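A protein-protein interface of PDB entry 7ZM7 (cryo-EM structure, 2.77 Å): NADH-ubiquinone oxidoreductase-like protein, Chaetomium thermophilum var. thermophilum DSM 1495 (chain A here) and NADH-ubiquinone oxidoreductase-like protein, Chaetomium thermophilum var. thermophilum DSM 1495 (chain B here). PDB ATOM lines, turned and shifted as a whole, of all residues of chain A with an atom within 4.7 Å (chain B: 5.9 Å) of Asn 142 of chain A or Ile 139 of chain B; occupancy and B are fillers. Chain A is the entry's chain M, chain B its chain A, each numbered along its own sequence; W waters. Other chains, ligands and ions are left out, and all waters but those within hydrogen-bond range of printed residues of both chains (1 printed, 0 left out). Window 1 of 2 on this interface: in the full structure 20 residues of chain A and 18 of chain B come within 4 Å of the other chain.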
ATOM      1  N   ILE A 129     -19.857  26.598  21.504  1.00  0.00           N
ATOM      2  CA  ILE A 129     -18.684  27.408  21.769  1.00  0.00           C
ATOM      3  C   ILE A 129     -18.084  27.836  20.443  1.00  0.00           C
ATOM      4  O   ILE A 129     -18.539  27.439  19.378  1.00  0.00           O
ATOM      5  CB  ILE A 129     -17.643  26.672  22.633  1.00  0.00           C
ATOM      6  CG1 ILE A 129     -17.210  25.369  21.979  1.00  0.00           C
ATOM      7  CG2 ILE A 129     -18.181  26.418  24.019  1.00  0.00           C
ATOM      8  CD1 ILE A 129     -15.837  24.969  22.347  1.00  0.00           C
ATOM      9  N   THR A 140      -8.846  22.408  18.259  1.00  0.00           N
ATOM     10  CA  THR A 140      -9.783  21.317  18.643  1.00  0.00           C
ATOM     11  C   THR A 140     -10.838  21.801  19.636  1.00  0.00           C
ATOM     12  O   THR A 140     -10.485  22.587  20.529  1.00  0.00           O
ATOM     13  CB  THR A 140      -9.037  20.123  19.246  1.00  0.00           C
ATOM     14  OG1 THR A 140      -8.407  20.561  20.449  1.00  0.00           O
ATOM     15  CG2 THR A 140      -8.003  19.540  18.311  1.00  0.00           C
ATOM     16  N   CYS A 141     -12.088  21.370  19.446  1.00  0.00           N
ATOM     17  CA  CYS A 141     -13.190  21.751  20.363  1.00  0.00           C
ATOM     18  C   CYS A 141     -12.870  21.224  21.762  1.00  0.00           C
ATOM     19  O   CYS A 141     -12.498  20.047  21.879  1.00  0.00           O
ATOM     20  CB  CYS A 141     -14.499  21.157  19.870  1.00  0.00           C
ATOM     21  SG  CYS A 141     -15.902  21.501  20.958  1.00  0.00           S
ATOM     22  N   ASN A 142     -12.991  22.076  22.780  1.00  0.00           N
ATOM     23  CA  ASN A 142     -12.636  21.676  24.165  1.00  0.00           C
ATOM     24  C   ASN A 142     -13.585  20.578  24.655  1.00  0.00           C
ATOM     25  O   ASN A 142     -13.113  19.666  25.354  1.00  0.00           O
ATOM     26  CB  ASN A 142     -12.548  22.894  25.083  1.00  0.00           C
ATOM     27  CG  ASN A 142     -11.343  23.760  24.791  1.00  0.00           C
ATOM     28  OD1 ASN A 142     -10.395  23.310  24.154  1.00  0.00           O
ATOM     29  ND2 ASN A 142     -11.370  24.997  25.255  1.00  0.00           N
ATOM     30  N   TYR A 143     -14.876  20.697  24.353  1.00  0.00           N
ATOM     31  CA  TYR A 143     -15.867  19.673  24.758  1.00  0.00           C
ATOM     32  C   TYR A 143     -15.775  18.345  23.999  1.00  0.00           C
ATOM     33  O   TYR A 143     -15.778  17.305  24.666  1.00  0.00           O
ATOM     34  CB  TYR A 143     -17.277  20.234  24.596  1.00  0.00           C
ATOM     35  CG  TYR A 143     -17.717  21.235  25.630  1.00  0.00           C
ATOM     36  CD1 TYR A 143     -18.279  20.823  26.825  1.00  0.00           C
ATOM     37  CD2 TYR A 143     -17.607  22.596  25.401  1.00  0.00           C
ATOM     38  CE1 TYR A 143     -18.704  21.734  27.775  1.00  0.00           C
ATOM     39  CE2 TYR A 143     -18.023  23.521  26.343  1.00  0.00           C
ATOM     40  CZ  TYR A 143     -18.573  23.088  27.534  1.00  0.00           C
ATOM     41  OH  TYR A 143     -18.990  23.992  28.465  1.00  0.00           O
ATOM     42  N   CYS A 144     -15.660  18.352  22.668  1.00  0.00           N
ATOM     43  CA  CYS A 144     -15.760  17.065  21.914  1.00  0.00           C
ATOM     44  C   CYS A 144     -14.454  16.606  21.263  1.00  0.00           C
ATOM     45  O   CYS A 144     -14.340  15.403  21.012  1.00  0.00           O
ATOM     46  CB  CYS A 144     -16.894  17.101  20.895  1.00  0.00           C
ATOM     47  SG  CYS A 144     -16.578  18.105  19.421  1.00  0.00           S
ATOM     48  N   LEU B 135     -19.235  29.692  26.606  1.00  0.00           N
ATOM     49  CA  LEU B 135     -20.061  28.828  27.425  1.00  0.00           C
ATOM     50  C   LEU B 135     -19.225  27.678  27.951  1.00  0.00           C
ATOM     51  O   LEU B 135     -19.440  26.535  27.565  1.00  0.00           O
ATOM     52  CB  LEU B 135     -21.256  28.314  26.623  1.00  0.00           C
ATOM     53  CG  LEU B 135     -22.578  29.073  26.683  1.00  0.00           C
ATOM     54  CD1 LEU B 135     -22.469  30.409  26.038  1.00  0.00           C
ATOM     55  CD2 LEU B 135     -23.632  28.275  26.013  1.00  0.00           C
ATOM     56  N   ASP B 136     -18.180  28.009  28.706  1.00  0.00           N
ATOM     57  CA  ASP B 136     -17.177  26.993  29.102  1.00  0.00           C
ATOM     58  C   ASP B 136     -17.172  26.773  30.606  1.00  0.00           C
ATOM     59  O   ASP B 136     -16.077  26.582  31.139  1.00  0.00           O
ATOM     60  CB  ASP B 136     -15.779  27.473  28.712  1.00  0.00           C
ATOM     61  CG  ASP B 136     -15.479  27.452  27.228  1.00  0.00           C
ATOM     62  OD1 ASP B 136     -16.297  26.910  26.474  1.00  0.00           O
ATOM     63  OD2 ASP B 136     -14.417  27.969  26.848  1.00  0.00           O
ATOM     64  N   CYS B 137     -18.333  26.727  31.253  1.00  0.00           N
ATOM     65  CA  CYS B 137     -18.325  26.625  32.733  1.00  0.00           C
ATOM     66  C   CYS B 137     -18.046  25.174  33.116  1.00  0.00           C
ATOM     67  O   CYS B 137     -17.270  24.988  34.066  1.00  0.00           O
ATOM     68  CB  CYS B 137     -19.651  27.076  33.338  1.00  0.00           C
ATOM     69  SG  CYS B 137     -19.879  28.871  33.379  1.00  0.00           S
ATOM     70  N   PRO B 138     -18.625  24.128  32.471  1.00  0.00           N
ATOM     71  CA  PRO B 138     -18.228  22.760  32.801  1.00  0.00           C
ATOM     72  C   PRO B 138     -16.761  22.438  32.582  1.00  0.00           C
ATOM     73  O   PRO B 138     -16.227  21.598  33.304  1.00  0.00           O
ATOM     74  CB  PRO B 138     -19.151  21.944  31.902  1.00  0.00           C
ATOM     75  CG  PRO B 138     -20.338  22.739  31.862  1.00  0.00           C
ATOM     76  CD  PRO B 138     -19.837  24.100  31.641  1.00  0.00           C
ATOM     77  N   ILE B 139     -16.079  23.075  31.630  1.00  0.00           N
ATOM     78  CA  ILE B 139     -14.671  22.793  31.366  1.00  0.00           C
ATOM     79  C   ILE B 139     -13.743  23.816  31.998  1.00  0.00           C
ATOM     80  O   ILE B 139     -12.533  23.754  31.777  1.00  0.00           O
ATOM     81  CB  ILE B 139     -14.401  22.711  29.850  1.00  0.00           C
ATOM     82  CG1 ILE B 139     -14.803  24.009  29.171  1.00  0.00           C
ATOM     83  CG2 ILE B 139     -15.169  21.606  29.217  1.00  0.00           C
ATOM     84  CD1 ILE B 139     -14.426  24.093  27.765  1.00  0.00           C
ATOM     85  N   CYS B 140     -14.301  24.811  32.693  1.00  0.00           N
ATOM     86  CA  CYS B 140     -13.503  25.901  33.323  1.00  0.00           C
ATOM     87  C   CYS B 140     -13.084  25.488  34.724  1.00  0.00           C
ATOM     88  O   CYS B 140     -13.889  24.872  35.426  1.00  0.00           O
ATOM     89  CB  CYS B 140     -14.337  27.169  33.475  1.00  0.00           C
ATOM     90  SG  CYS B 140     -13.429  28.701  33.799  1.00  0.00           S
ATOM     91  N   ASP B 141     -11.859  25.827  35.105  1.00  0.00           N
ATOM     92  CA  ASP B 141     -11.387  25.547  36.448  1.00  0.00           C
ATOM     93  C   ASP B 141     -11.889  26.536  37.460  1.00  0.00           C
ATOM     94  O   ASP B 141     -11.898  26.225  38.645  1.00  0.00           O
ATOM     95  CB  ASP B 141      -9.878  25.535  36.488  1.00  0.00           C
ATOM     96  CG  ASP B 141      -9.325  24.417  35.712  1.00  0.00           C
ATOM     97  OD1 ASP B 141      -9.893  23.322  35.846  1.00  0.00           O
ATOM     98  OD2 ASP B 141      -8.349  24.629  34.964  1.00  0.00           O
ATOM     99  N   SER B 183      -6.890  30.267  28.829  1.00  0.00           N
ATOM    100  CA  SER B 183      -8.139  30.030  28.064  1.00  0.00           C
ATOM    101  C   SER B 183      -8.618  31.461  27.919  1.00  0.00           C
ATOM    102  O   SER B 183      -9.527  31.840  28.659  1.00  0.00           O
ATOM    103  CB  SER B 183      -9.098  29.211  28.850  1.00  0.00           C
ATOM    104  OG  SER B 183      -9.984  28.526  27.988  1.00  0.00           O
ATOM    105  N   ARG B 186     -12.090  33.670  27.851  1.00  0.00           N
ATOM    106  CA  ARG B 186     -12.784  33.991  29.077  1.00  0.00           C
ATOM    107  C   ARG B 186     -12.430  35.360  29.613  1.00  0.00           C
ATOM    108  O   ARG B 186     -13.096  35.819  30.541  1.00  0.00           O
ATOM    109  CB  ARG B 186     -12.486  32.915  30.122  1.00  0.00           C
ATOM    110  CG  ARG B 186     -12.820  31.519  29.650  1.00  0.00           C
ATOM    111  CD  ARG B 186     -12.267  30.421  30.508  1.00  0.00           C
ATOM    112  NE  ARG B 186     -12.633  29.116  29.975  1.00  0.00           N
ATOM    113  CZ  ARG B 186     -12.112  27.963  30.366  1.00  0.00           C
ATOM    114  NH1 ARG B 186     -11.183  27.939  31.295  1.00  0.00           N
ATOM    115  NH2 ARG B 186     -12.512  26.842  29.809  1.00  0.00           N
ATOM    116  N   PHE B 249      -7.216  20.113  35.992  1.00  0.00           N
ATOM    117  CA  PHE B 249      -8.668  19.795  35.926  1.00  0.00           C
ATOM    118  C   PHE B 249      -8.951  18.822  37.050  1.00  0.00           C
ATOM    119  O   PHE B 249      -9.990  18.159  37.029  1.00  0.00           O
ATOM    120  CB  PHE B 249      -9.003  19.117  34.596  1.00  0.00           C
ATOM    121  CG  PHE B 249      -8.594  19.827  33.330  1.00  0.00           C
ATOM    122  CD1 PHE B 249      -9.131  21.060  32.993  1.00  0.00           C
ATOM    123  CD2 PHE B 249      -7.717  19.228  32.442  1.00  0.00           C
ATOM    124  CE1 PHE B 249      -8.771  21.692  31.815  1.00  0.00           C
ATOM    125  CE2 PHE B 249      -7.362  19.860  31.262  1.00  0.00           C
ATOM    126  CZ  PHE B 249      -7.889  21.090  30.952  1.00  0.00           C
ATOM    127  N   ARG B 252     -12.781  20.229  42.010  1.00  0.00           N
ATOM    128  CA  ARG B 252     -13.811  21.290  42.032  1.00  0.00           C
ATOM    129  C   ARG B 252     -13.728  21.975  43.405  1.00  0.00           C
ATOM    130  O   ARG B 252     -13.508  21.267  44.381  1.00  0.00           O
ATOM    131  CB  ARG B 252     -15.174  20.693  41.684  1.00  0.00           C
ATOM    132  CG  ARG B 252     -15.383  20.506  40.191  1.00  0.00           C
ATOM    133  CD  ARG B 252     -15.315  21.843  39.495  1.00  0.00           C
ATOM    134  NE  ARG B 252     -15.790  21.733  38.128  1.00  0.00           N
ATOM    135  CZ  ARG B 252     -15.723  22.707  37.240  1.00  0.00           C
ATOM    136  NH1 ARG B 252     -15.200  23.868  37.580  1.00  0.00           N
ATOM    137  NH2 ARG B 252     -16.172  22.516  36.017  1.00  0.00           N
HETATM  138  O   HOH W   1      -8.985  26.464  26.614  1.00  0.00           O
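Printed residues of chain B within 4 Å of Ile 129 of chain A: Leu 135 and Asp 136. Printed residues of chain B within 4 Å of Asn 142 of chain A: Ile 139 (3.5 Å). Of the printed residues of chain B, Tyr 143 of chain A touches Leu 135 (2.7 Å), Asp 136 (3.6 Å), Cys 137 (3.96 Å), Pro 138 (3.3 Å) and Ile 139 (3.8 Å). Cys 144 of chain A touches none of the printed residues of chain B. Printed residues of chain A within 4 Å of Cys 137 of chain B: Tyr 143 (3.96 Å). Of the printed residues of chain A, Pro 138 of chain B touches Tyr 143. Of chain A, only Asn 142 and Tyr 143 come within 4 Å of Ile 139 of chain B. Asp 141 of chain B touches none of the printed residues of chain A. The nearest printed residue of chain A that does not touch Cys 137 of chain B is Ile 129 of chain A (7.2 Å).
OH of Tyr 143 of chain A sits at hydrogen-bond distance from O of Leu 135 of chain B (2.7 Å).
Water W1 bridges the side-chain hydroxyl (OG) of Ser 183 of chain B (2.7 Å) and the side-chain amide nitrogen (ND2) of Asn 142 of chain A (3.1 Å).
Hydrophobic or aromatic side chains of chain B within 4 Å of the printed part of chain A: Pro 138 and Ile 139. Among the printed residues, 8 pairs touch across the chains.
OD2 of Asp 136 of chain B is in salt-bridge range of NH2 of Arg 186 of chain B (3.7 Å). O of Cys 137 of chain B lies within hydrogen-bond range of NH2 of Arg 252 of chain B (3.3 Å). The backbone carbonyl oxygen (O) of Pro 138 of chain B lies within hydrogen-bond range of the guanidinium group (NH2) of Arg 252 of chain B, 2.9 Å away. N of Tyr 143 of chain A lies close to SG of Cys 141 of chain A (3.6 Å).
Among the printed residues, merely in contact across the chains: Ile 129 of chain A with Leu 135 of chain B (3.8 Å), Ile 129 of chain A with Asp 136 of chain B (3.1 Å), Asn 142 of chain A with Ile 139 of chain B (3.5 Å), Tyr 143 of chain A with Asp 136 of chain B (3.6 Å), Tyr 143 of chain A with Cys 137 of chain B (3.96 Å), Tyr 143 of chain A with Pro 138 of chain B (3.3 Å) and Tyr 143 of chain A with Ile 139 of chain B (3.8 Å).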
